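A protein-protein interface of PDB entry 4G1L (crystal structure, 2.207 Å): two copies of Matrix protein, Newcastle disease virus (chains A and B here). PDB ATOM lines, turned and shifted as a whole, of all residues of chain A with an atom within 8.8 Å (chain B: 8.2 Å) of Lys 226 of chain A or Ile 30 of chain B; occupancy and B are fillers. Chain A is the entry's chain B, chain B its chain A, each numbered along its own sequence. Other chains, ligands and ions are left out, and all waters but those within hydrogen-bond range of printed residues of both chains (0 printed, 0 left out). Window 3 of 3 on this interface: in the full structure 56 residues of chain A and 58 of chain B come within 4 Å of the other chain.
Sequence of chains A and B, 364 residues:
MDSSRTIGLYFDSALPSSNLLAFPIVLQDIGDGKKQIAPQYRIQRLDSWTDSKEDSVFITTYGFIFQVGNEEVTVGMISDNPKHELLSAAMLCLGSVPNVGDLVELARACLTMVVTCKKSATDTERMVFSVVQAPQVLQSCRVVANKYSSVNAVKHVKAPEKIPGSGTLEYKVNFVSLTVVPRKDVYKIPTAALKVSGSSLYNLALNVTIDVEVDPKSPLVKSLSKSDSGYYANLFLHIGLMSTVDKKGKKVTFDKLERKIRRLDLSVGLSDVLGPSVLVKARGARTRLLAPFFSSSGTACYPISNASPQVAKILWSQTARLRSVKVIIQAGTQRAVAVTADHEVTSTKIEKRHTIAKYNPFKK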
ATOM      1  N   ASP A 215     -10.700  39.667  21.151  1.00  0.00           N
ATOM      2  CA  ASP A 215     -10.798  39.069  19.841  1.00  0.00           C
ATOM      3  C   ASP A 215      -9.976  37.780  19.790  1.00  0.00           C
ATOM      4  O   ASP A 215      -8.863  37.752  20.320  1.00  0.00           O
ATOM      5  CB  ASP A 215     -10.260  40.058  18.814  1.00  0.00           C
ATOM      6  CG  ASP A 215     -10.757  39.762  17.436  1.00  0.00           C
ATOM      7  OD1 ASP A 215     -11.825  40.328  17.072  1.00  0.00           O
ATOM      8  OD2 ASP A 215     -10.107  38.934  16.751  1.00  0.00           O
ATOM      9  N   PRO A 216     -10.502  36.716  19.141  1.00  0.00           N
ATOM     10  CA  PRO A 216      -9.797  35.419  19.128  1.00  0.00           C
ATOM     11  C   PRO A 216      -8.464  35.442  18.366  1.00  0.00           C
ATOM     12  O   PRO A 216      -7.538  34.699  18.722  1.00  0.00           O
ATOM     13  CB  PRO A 216     -10.802  34.468  18.475  1.00  0.00           C
ATOM     14  CG  PRO A 216     -12.123  35.111  18.684  1.00  0.00           C
ATOM     15  CD  PRO A 216     -11.847  36.591  18.561  1.00  0.00           C
ATOM     16  N   LYS A 217      -8.357  36.305  17.355  1.00  0.00           N
ATOM     17  CA  LYS A 217      -7.089  36.465  16.642  1.00  0.00           C
ATOM     18  C   LYS A 217      -5.961  37.058  17.526  1.00  0.00           C
ATOM     19  O   LYS A 217      -4.780  36.777  17.321  1.00  0.00           O
ATOM     20  CB  LYS A 217      -7.281  37.244  15.324  1.00  0.00           C
ATOM     21  CG  LYS A 217      -7.517  38.747  15.455  1.00  0.00           C
ATOM     22  CD  LYS A 217      -7.814  39.331  14.082  1.00  0.00           C
ATOM     23  CE  LYS A 217      -7.764  40.854  14.064  1.00  0.00           C
ATOM     24  NZ  LYS A 217      -7.573  41.351  12.673  1.00  0.00           N
ATOM     25  N   SER A 218      -6.344  37.853  18.519  1.00  0.00           N
ATOM     26  CA  SER A 218      -5.401  38.456  19.456  1.00  0.00           C
ATOM     27  C   SER A 218      -4.538  37.421  20.194  1.00  0.00           C
ATOM     28  O   SER A 218      -5.070  36.460  20.757  1.00  0.00           O
ATOM     29  CB  SER A 218      -6.172  39.311  20.458  1.00  0.00           C
ATOM     30  OG  SER A 218      -5.334  39.721  21.502  1.00  0.00           O
ATOM     31  N   LEU A 220      -3.357  37.449  22.997  1.00  0.00           N
ATOM     32  CA  LEU A 220      -3.708  37.441  24.429  1.00  0.00           C
ATOM     33  C   LEU A 220      -4.549  36.235  24.862  1.00  0.00           C
ATOM     34  O   LEU A 220      -4.504  35.807  26.024  1.00  0.00           O
ATOM     35  CB  LEU A 220      -4.425  38.741  24.801  1.00  0.00           C
ATOM     36  CG  LEU A 220      -3.592  40.036  24.885  1.00  0.00           C
ATOM     37  CD1 LEU A 220      -4.498  41.238  24.634  1.00  0.00           C
ATOM     38  CD2 LEU A 220      -2.873  40.198  26.225  1.00  0.00           C
ATOM     39  N   VAL A 221      -5.312  35.699  23.913  1.00  0.00           N
ATOM     40  CA  VAL A 221      -6.103  34.472  24.102  1.00  0.00           C
ATOM     41  C   VAL A 221      -5.285  33.314  24.713  1.00  0.00           C
ATOM     42  O   VAL A 221      -5.827  32.467  25.427  1.00  0.00           O
ATOM     43  CB  VAL A 221      -6.697  34.027  22.739  1.00  0.00           C
ATOM     44  CG1 VAL A 221      -7.490  32.735  22.861  1.00  0.00           C
ATOM     45  CG2 VAL A 221      -7.564  35.127  22.151  1.00  0.00           C
ATOM     46  N   LYS A 222      -3.983  33.285  24.430  1.00  0.00           N
ATOM     47  CA  LYS A 222      -3.169  32.111  24.734  1.00  0.00           C
ATOM     48  C   LYS A 222      -3.168  31.895  26.239  1.00  0.00           C
ATOM     49  O   LYS A 222      -3.224  30.763  26.722  1.00  0.00           O
ATOM     50  CB  LYS A 222      -1.709  32.240  24.232  1.00  0.00           C
ATOM     51  CG  LYS A 222      -1.456  32.657  22.785  1.00  0.00           C
ATOM     52  CD  LYS A 222      -1.557  31.553  21.736  1.00  0.00           C
ATOM     53  CE  LYS A 222      -0.759  31.896  20.465  1.00  0.00           C
ATOM     54  NZ  LYS A 222      -0.652  33.341  20.053  1.00  0.00           N
ATOM     55  N   SER A 223      -3.116  32.984  26.988  1.00  0.00           N
ATOM     56  CA  SER A 223      -2.948  32.830  28.408  1.00  0.00           C
ATOM     57  C   SER A 223      -4.296  32.841  29.147  1.00  0.00           C
ATOM     58  O   SER A 223      -4.345  32.805  30.376  1.00  0.00           O
ATOM     59  CB  SER A 223      -1.913  33.826  28.938  1.00  0.00           C
ATOM     60  OG  SER A 223      -2.496  35.084  29.193  1.00  0.00           O
ATOM     61  N   LEU A 224      -5.397  32.798  28.400  1.00  0.00           N
ATOM     62  CA  LEU A 224      -6.713  32.891  29.037  1.00  0.00           C
ATOM     63  C   LEU A 224      -7.458  31.545  29.075  1.00  0.00           C
ATOM     64  O   LEU A 224      -7.165  30.648  28.302  1.00  0.00           O
ATOM     65  CB  LEU A 224      -7.559  33.999  28.388  1.00  0.00           C
ATOM     66  CG  LEU A 224      -7.059  35.456  28.500  1.00  0.00           C
ATOM     67  CD1 LEU A 224      -7.835  36.407  27.568  1.00  0.00           C
ATOM     68  CD2 LEU A 224      -7.078  35.982  29.918  1.00  0.00           C
ATOM     69  N   SER A 225      -8.410  31.418  29.989  1.00  0.00           N
ATOM     70  CA  SER A 225      -9.368  30.312  29.936  1.00  0.00           C
ATOM     71  C   SER A 225     -10.538  30.437  28.901  1.00  0.00           C
ATOM     72  O   SER A 225     -11.255  31.429  28.843  1.00  0.00           O
ATOM     73  CB  SER A 225      -9.892  30.024  31.335  1.00  0.00           C
ATOM     74  OG  SER A 225      -8.854  29.497  32.139  1.00  0.00           O
ATOM     75  N   LYS A 226     -10.706  29.403  28.091  1.00  0.00           N
ATOM     76  CA  LYS A 226     -11.785  29.365  27.104  1.00  0.00           C
ATOM     77  C   LYS A 226     -13.129  29.165  27.819  1.00  0.00           C
ATOM     78  O   LYS A 226     -13.327  28.218  28.590  1.00  0.00           O
ATOM     79  CB  LYS A 226     -11.515  28.312  25.995  1.00  0.00           C
ATOM     80  CG  LYS A 226     -10.130  28.451  25.326  1.00  0.00           C
ATOM     81  CD  LYS A 226     -10.020  27.740  23.963  1.00  0.00           C
ATOM     82  CE  LYS A 226      -8.705  28.043  23.224  1.00  0.00           C
ATOM     83  NZ  LYS A 226      -8.723  29.239  22.312  1.00  0.00           N
ATOM     84  N   SER A 227     -14.025  30.118  27.605  1.00  0.00           N
ATOM     85  CA  SER A 227     -15.364  30.050  28.141  1.00  0.00           C
ATOM     86  C   SER A 227     -16.355  29.615  27.066  1.00  0.00           C
ATOM     87  O   SER A 227     -16.115  29.724  25.856  1.00  0.00           O
ATOM     88  CB  SER A 227     -15.749  31.397  28.745  1.00  0.00           C
ATOM     89  OG  SER A 227     -17.089  31.738  28.470  1.00  0.00           O
ATOM     90  N   ASP A 228     -17.479  29.108  27.540  1.00  0.00           N
ATOM     91  CA  ASP A 228     -18.589  28.761  26.686  1.00  0.00           C
ATOM     92  C   ASP A 228     -19.026  30.043  25.957  1.00  0.00           C
ATOM     93  O   ASP A 228     -19.208  30.048  24.741  1.00  0.00           O
ATOM     94  CB  ASP A 228     -19.661  28.103  27.564  1.00  0.00           C
ATOM     95  CG  ASP A 228     -19.023  27.264  28.713  1.00  0.00           C
ATOM     96  OD1 ASP A 228     -18.579  26.108  28.469  1.00  0.00           O
ATOM     97  OD2 ASP A 228     -18.914  27.794  29.850  1.00  0.00           O
ATOM     98  N   SER A 229     -19.091  31.147  26.698  1.00  0.00           N
ATOM     99  CA  SER A 229     -19.350  32.475  26.126  1.00  0.00           C
ATOM    100  C   SER A 229     -18.120  33.127  25.468  1.00  0.00           C
ATOM    101  O   SER A 229     -18.166  33.487  24.292  1.00  0.00           O
ATOM    102  CB  SER A 229     -19.900  33.388  27.221  1.00  0.00           C
ATOM    103  OG  SER A 229     -19.483  32.889  28.490  1.00  0.00           O
ATOM    104  N   GLY A 230     -17.032  33.282  26.225  1.00  0.00           N
ATOM    105  CA  GLY A 230     -15.853  33.993  25.742  1.00  0.00           C
ATOM    106  C   GLY A 230     -14.576  33.577  26.442  1.00  0.00           C
ATOM    107  O   GLY A 230     -14.266  32.393  26.517  1.00  0.00           O
ATOM    108  N   TYR A 231     -13.825  34.552  26.943  1.00  0.00           N
ATOM    109  CA  TYR A 231     -12.569  34.258  27.591  1.00  0.00           C
ATOM    110  C   TYR A 231     -12.633  34.749  28.966  1.00  0.00           C
ATOM    111  O   TYR A 231     -13.238  35.785  29.222  1.00  0.00           O
ATOM    112  CB  TYR A 231     -11.392  34.886  26.852  1.00  0.00           C
ATOM    113  CG  TYR A 231     -11.230  34.230  25.506  1.00  0.00           C
ATOM    114  CD1 TYR A 231     -10.691  32.943  25.408  1.00  0.00           C
ATOM    115  CD2 TYR A 231     -11.689  34.846  24.354  1.00  0.00           C
ATOM    116  CE1 TYR A 231     -10.577  32.315  24.192  1.00  0.00           C
ATOM    117  CE2 TYR A 231     -11.576  34.221  23.120  1.00  0.00           C
ATOM    118  CZ  TYR A 231     -11.023  32.956  23.053  1.00  0.00           C
ATOM    119  OH  TYR A 231     -10.900  32.335  21.843  1.00  0.00           O
ATOM    120  N   TYR A 232     -12.050  33.976  29.878  1.00  0.00           N
ATOM    121  CA  TYR A 232     -11.907  34.483  31.189  1.00  0.00           C
ATOM    122  C   TYR A 232     -10.479  34.437  31.763  1.00  0.00           C
ATOM    123  O   TYR A 232      -9.559  33.884  31.162  1.00  0.00           O
ATOM    124  CB  TYR A 232     -13.002  33.947  32.084  1.00  0.00           C
ATOM    125  CG  TYR A 232     -12.941  32.483  32.417  1.00  0.00           C
ATOM    126  CD1 TYR A 232     -12.282  32.059  33.543  1.00  0.00           C
ATOM    127  CD2 TYR A 232     -13.608  31.516  31.635  1.00  0.00           C
ATOM    128  CE1 TYR A 232     -12.242  30.727  33.899  1.00  0.00           C
ATOM    129  CE2 TYR A 232     -13.566  30.163  31.987  1.00  0.00           C
ATOM    130  CZ  TYR A 232     -12.875  29.788  33.130  1.00  0.00           C
ATOM    131  OH  TYR A 232     -12.781  28.490  33.535  1.00  0.00           O
ATOM    132  N   ALA A 233     -10.294  35.117  32.887  1.00  0.00           N
ATOM    133  CA  ALA A 233      -9.026  35.136  33.604  1.00  0.00           C
ATOM    134  C   ALA A 233      -9.295  34.679  35.037  1.00  0.00           C
ATOM    135  O   ALA A 233     -10.337  34.993  35.573  1.00  0.00           O
ATOM    136  CB  ALA A 233      -8.444  36.544  33.569  1.00  0.00           C
ATOM    137  N   ASN A 234      -8.382  33.913  35.633  1.00  0.00           N
ATOM    138  CA  ASN A 234      -8.536  33.395  37.006  1.00  0.00           C
ATOM    139  C   ASN A 234      -7.657  34.206  37.951  1.00  0.00           C
ATOM    140  O   ASN A 234      -6.517  34.502  37.603  1.00  0.00           O
ATOM    141  CB  ASN A 234      -8.058  31.947  37.076  1.00  0.00           C
ATOM    142  CG  ASN A 234      -8.894  31.002  36.234  1.00  0.00           C
ATOM    143  OD1 ASN A 234      -9.965  30.585  36.652  1.00  0.00           O
ATOM    144  ND2 ASN A 234      -8.383  30.623  35.059  1.00  0.00           N
ATOM    145  N   ARG A 323     -17.007  37.515  36.287  1.00  0.00           N
ATOM    146  CA  ARG A 323     -17.744  36.349  35.833  1.00  0.00           C
ATOM    147  C   ARG A 323     -18.346  35.679  37.051  1.00  0.00           C
ATOM    148  O   ARG A 323     -19.491  35.255  37.024  1.00  0.00           O
ATOM    149  CB  ARG A 323     -16.809  35.362  35.157  1.00  0.00           C
ATOM    150  CG  ARG A 323     -17.506  34.111  34.637  1.00  0.00           C
ATOM    151  CD  ARG A 323     -16.498  33.140  34.067  1.00  0.00           C
ATOM    152  NE  ARG A 323     -17.113  32.242  33.116  1.00  0.00           N
ATOM    153  CZ  ARG A 323     -17.357  30.963  33.354  1.00  0.00           C
ATOM    154  NH1 ARG A 323     -17.022  30.427  34.527  1.00  0.00           N
ATOM    155  NH2 ARG A 323     -17.935  30.223  32.416  1.00  0.00           N
ATOM    156  N   PHE B  23       4.770  27.140  27.187  1.00  0.00           N
ATOM    157  CA  PHE B  23       3.338  26.901  27.269  1.00  0.00           C
ATOM    158  C   PHE B  23       2.649  27.738  28.354  1.00  0.00           C
ATOM    159  O   PHE B  23       3.091  27.744  29.501  1.00  0.00           O
ATOM    160  CB  PHE B  23       3.044  25.414  27.429  1.00  0.00           C
ATOM    161  CG  PHE B  23       1.634  25.081  27.126  1.00  0.00           C
ATOM    162  CD1 PHE B  23       1.256  24.777  25.827  1.00  0.00           C
ATOM    163  CD2 PHE B  23       0.670  25.148  28.123  1.00  0.00           C
ATOM    164  CE1 PHE B  23      -0.062  24.484  25.532  1.00  0.00           C
ATOM    165  CE2 PHE B  23      -0.642  24.881  27.839  1.00  0.00           C
ATOM    166  CZ  PHE B  23      -1.006  24.533  26.544  1.00  0.00           C
ATOM    167  N   PRO B  24       1.551  28.443  27.988  1.00  0.00           N
ATOM    168  CA  PRO B  24       0.772  28.304  26.754  1.00  0.00           C
ATOM    169  C   PRO B  24       1.101  29.291  25.653  1.00  0.00           C
ATOM    170  O   PRO B  24       0.320  29.426  24.708  1.00  0.00           O
ATOM    171  CB  PRO B  24      -0.642  28.585  27.244  1.00  0.00           C
ATOM    172  CG  PRO B  24      -0.441  29.648  28.299  1.00  0.00           C
ATOM    173  CD  PRO B  24       0.970  29.498  28.839  1.00  0.00           C
ATOM    174  N   VAL B  26       2.834  29.498  22.970  1.00  0.00           N
ATOM    175  CA  VAL B  26       3.505  28.676  21.970  1.00  0.00           C
ATOM    176  C   VAL B  26       2.464  28.484  20.883  1.00  0.00           C
ATOM    177  O   VAL B  26       1.268  28.643  21.134  1.00  0.00           O
ATOM    178  CB  VAL B  26       3.911  27.283  22.542  1.00  0.00           C
ATOM    179  CG1 VAL B  26       4.906  27.423  23.681  1.00  0.00           C
ATOM    180  CG2 VAL B  26       2.690  26.506  23.029  1.00  0.00           C
ATOM    181  N   LEU B  27       2.904  28.127  19.683  1.00  0.00           N
ATOM    182  CA  LEU B  27       1.993  28.021  18.546  1.00  0.00           C
ATOM    183  C   LEU B  27       0.794  27.061  18.746  1.00  0.00           C
ATOM    184  O   LEU B  27      -0.365  27.450  18.550  1.00  0.00           O
ATOM    185  CB  LEU B  27       2.793  27.705  17.281  1.00  0.00           C
ATOM    186  CG  LEU B  27       3.627  28.935  16.902  1.00  0.00           C
ATOM    187  CD1 LEU B  27       4.833  28.583  16.037  1.00  0.00           C
ATOM    188  CD2 LEU B  27       2.762  30.014  16.253  1.00  0.00           C
ATOM    189  N   GLN B  28       1.081  25.829  19.157  1.00  0.00           N
ATOM    190  CA  GLN B  28       0.064  24.784  19.305  1.00  0.00           C
ATOM    191  C   GLN B  28      -0.409  24.715  20.776  1.00  0.00           C
ATOM    192  O   GLN B  28       0.004  23.838  21.532  1.00  0.00           O
ATOM    193  CB  GLN B  28       0.623  23.457  18.716  1.00  0.00           C
ATOM    194  CG  GLN B  28      -0.050  22.125  19.068  1.00  0.00           C
ATOM    195  CD  GLN B  28       0.879  21.163  19.824  1.00  0.00           C
ATOM    196  OE1 GLN B  28       0.560  20.702  20.925  1.00  0.00           O
ATOM    197  NE2 GLN B  28       2.032  20.857  19.230  1.00  0.00           N
ATOM    198  N   ASP B  29      -1.273  25.664  21.162  1.00  0.00           N
ATOM    199  CA  ASP B  29      -1.678  25.879  22.582  1.00  0.00           C
ATOM    200  C   ASP B  29      -2.987  25.198  23.074  1.00  0.00           C
ATOM    201  O   ASP B  29      -3.234  25.106  24.282  1.00  0.00           O
ATOM    202  CB  ASP B  29      -1.656  27.390  22.942  1.00  0.00           C
ATOM    203  CG  ASP B  29      -3.065  28.019  23.091  1.00  0.00           C
ATOM    204  OD1 ASP B  29      -3.521  28.204  24.256  1.00  0.00           O
ATOM    205  OD2 ASP B  29      -3.701  28.354  22.055  1.00  0.00           O
ATOM    206  N   ILE B  30      -3.823  24.730  22.152  1.00  0.00           N
ATOM    207  CA  ILE B  30      -5.059  24.051  22.540  1.00  0.00           C
ATOM    208  C   ILE B  30      -4.741  22.599  22.947  1.00  0.00           C
ATOM    209  O   ILE B  30      -4.875  22.246  24.119  1.00  0.00           O
ATOM    210  CB  ILE B  30      -6.188  24.190  21.470  1.00  0.00           C
ATOM    211  CG1 ILE B  30      -6.802  25.601  21.494  1.00  0.00           C
ATOM    212  CG2 ILE B  30      -7.299  23.168  21.673  1.00  0.00           C
ATOM    213  CD1 ILE B  30      -6.170  26.597  20.542  1.00  0.00           C
ATOM    214  N   GLY B  31      -4.287  21.780  21.996  1.00  0.00           N
ATOM    215  CA  GLY B  31      -3.929  20.386  22.284  1.00  0.00           C
ATOM    216  C   GLY B  31      -2.543  20.042  21.782  1.00  0.00           C
ATOM    217  O   GLY B  31      -2.101  20.586  20.770  1.00  0.00           O
ATOM    218  N   HIS B  84      -6.873  14.752  31.300  1.00  0.00           N
ATOM    219  CA  HIS B  84      -5.674  15.511  31.661  1.00  0.00           C
ATOM    220  C   HIS B  84      -5.474  16.769  30.829  1.00  0.00           C
ATOM    221  O   HIS B  84      -5.097  16.675  29.658  1.00  0.00           O
ATOM    222  CB  HIS B  84      -4.451  14.635  31.479  1.00  0.00           C
ATOM    223  CG  HIS B  84      -4.000  13.911  32.721  1.00  0.00           C
ATOM    224  ND1 HIS B  84      -4.852  13.379  33.596  1.00  0.00           N
ATOM    225  CD2 HIS B  84      -2.720  13.613  33.193  1.00  0.00           C
ATOM    226  CE1 HIS B  84      -4.168  12.781  34.589  1.00  0.00           C
ATOM    227  NE2 HIS B  84      -2.863  12.930  34.342  1.00  0.00           N
ATOM    228  N   GLU B  85      -5.608  17.963  31.396  1.00  0.00           N
ATOM    229  CA  GLU B  85      -5.404  19.137  30.553  1.00  0.00           C
ATOM    230  C   GLU B  85      -4.246  20.057  30.883  1.00  0.00           C
ATOM    231  O   GLU B  85      -4.087  20.481  32.007  1.00  0.00           O
ATOM    232  CB  GLU B  85      -6.665  19.962  30.367  1.00  0.00           C
ATOM    233  CG  GLU B  85      -6.510  20.955  29.229  1.00  0.00           C
ATOM    234  CD  GLU B  85      -7.465  22.141  29.286  1.00  0.00           C
ATOM    235  OE1 GLU B  85      -8.616  21.988  29.753  1.00  0.00           O
ATOM    236  OE2 GLU B  85      -7.068  23.234  28.831  1.00  0.00           O
ATOM    237  N   LEU B  86      -3.470  20.349  29.842  1.00  0.00           N
ATOM    238  CA  LEU B  86      -2.268  21.179  29.914  1.00  0.00           C
ATOM    239  C   LEU B  86      -2.651  22.644  30.067  1.00  0.00           C
ATOM    240  O   LEU B  86      -3.195  23.250  29.144  1.00  0.00           O
ATOM    241  CB  LEU B  86      -1.375  21.007  28.663  1.00  0.00           C
ATOM    242  CG  LEU B  86       0.091  21.531  28.754  1.00  0.00           C
ATOM    243  CD1 LEU B  86       0.832  21.047  30.004  1.00  0.00           C
ATOM    244  CD2 LEU B  86       0.946  21.253  27.507  1.00  0.00           C
ATOM    245  N   LEU B  87      -2.382  23.196  31.245  1.00  0.00           N
ATOM    246  CA  LEU B  87      -2.613  24.619  31.500  1.00  0.00           C
ATOM    247  C   LEU B  87      -1.350  25.442  31.338  1.00  0.00           C
ATOM    248  O   LEU B  87      -1.376  26.410  30.605  1.00  0.00           O
ATOM    249  CB  LEU B  87      -3.169  24.862  32.897  1.00  0.00           C
ATOM    250  CG  LEU B  87      -4.390  24.071  33.356  1.00  0.00           C
ATOM    251  CD1 LEU B  87      -4.679  24.453  34.792  1.00  0.00           C
ATOM    252  CD2 LEU B  87      -5.596  24.304  32.466  1.00  0.00           C
ATOM    253  N   LYS B 162      -4.303  31.476  34.065  1.00  0.00           N
ATOM    254  CA  LYS B 162      -4.851  30.267  33.423  1.00  0.00           C
ATOM    255  C   LYS B 162      -5.133  29.161  34.425  1.00  0.00           C
ATOM    256  O   LYS B 162      -5.812  28.204  34.118  1.00  0.00           O
ATOM    257  CB  LYS B 162      -3.911  29.781  32.311  1.00  0.00           C
ATOM    258  CG  LYS B 162      -4.610  29.149  31.122  1.00  0.00           C
ATOM    259  CD  LYS B 162      -3.795  29.329  29.839  1.00  0.00           C
ATOM    260  CE  LYS B 162      -4.060  28.241  28.824  1.00  0.00           C
ATOM    261  NZ  LYS B 162      -4.907  28.748  27.710  1.00  0.00           N
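The side-chain amino group (NZ) of Lys 162 of chain B lies within hydrogen-bond range of the backbone carbonyl oxygen (O) of Lys 222 of chain A, 2.8 Å away.
The side-chain amino group (NZ) of Lys 162 of chain B lies within hydrogen-bond range of the backbone carbonyl oxygen (O) of Leu 224 of chain A (3.0 Å).
Printed residues of chain B within 4 Å of Lys 226 of chain A: Ile 30 (3.5 Å).
Of chain A, only Lys 226 (3.5 Å) comes within 4 Å of Ile 30 of chain B.
No residue of chain A comes within 4 Å of Gly 31 of chain B.
Of the printed residues of chain B, Ser 225 of chain A touches Lys 162.
Printed residues of chain B within 4 Å of Ser 223 of chain A: Lys 162.
Ser 218 of chain A touches none of the printed residues of chain B.
His 84 of chain B touches none of the printed residues of chain A.
The nearest residue of chain A that does not touch Ile 30 of chain B is Val 221 of chain A (6.7 Å).
Among the printed residues, merely in contact across the chains: Lys 222 of chain A with Pro 24 of chain B (3.4 Å), Lys 222 of chain A with Val 26 of chain B (3.9 Å), Lys 222 of chain A with Asp 29 of chain B (3.6 Å), Ser 223 of chain A with Lys 162 of chain B (3.6 Å), Ser 225 of chain A with Lys 162 of chain B (3.9 Å), Lys 226 of chain A with Ile 30 of chain B (3.5 Å) and Asn 234 of chain A with Lys 162 of chain B (3.6 Å).
No position is printed for both chains.
The side-chain amino group (NZ) of Lys 162 of chain B lies within salt-bridge range of the side-chain carboxylate (OD1) of Asp 29 of chain B (3.8 Å).
The backbone NH of Tyr 232 of chain A lies within hydrogen-bond range of the backbone carbonyl oxygen of Ser 225 of chain A, at 2.9 Å.
The side-chain hydroxyl of Ser 225 of chain A is in hydrogen-bond range of the side-chain amide nitrogen of Asn 234 of chain A (3.2 Å).
Among the printed residues, no Asp or Glu carboxylate lies within 4 Å of a Lys or Arg side-chain nitrogen of the other chain.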
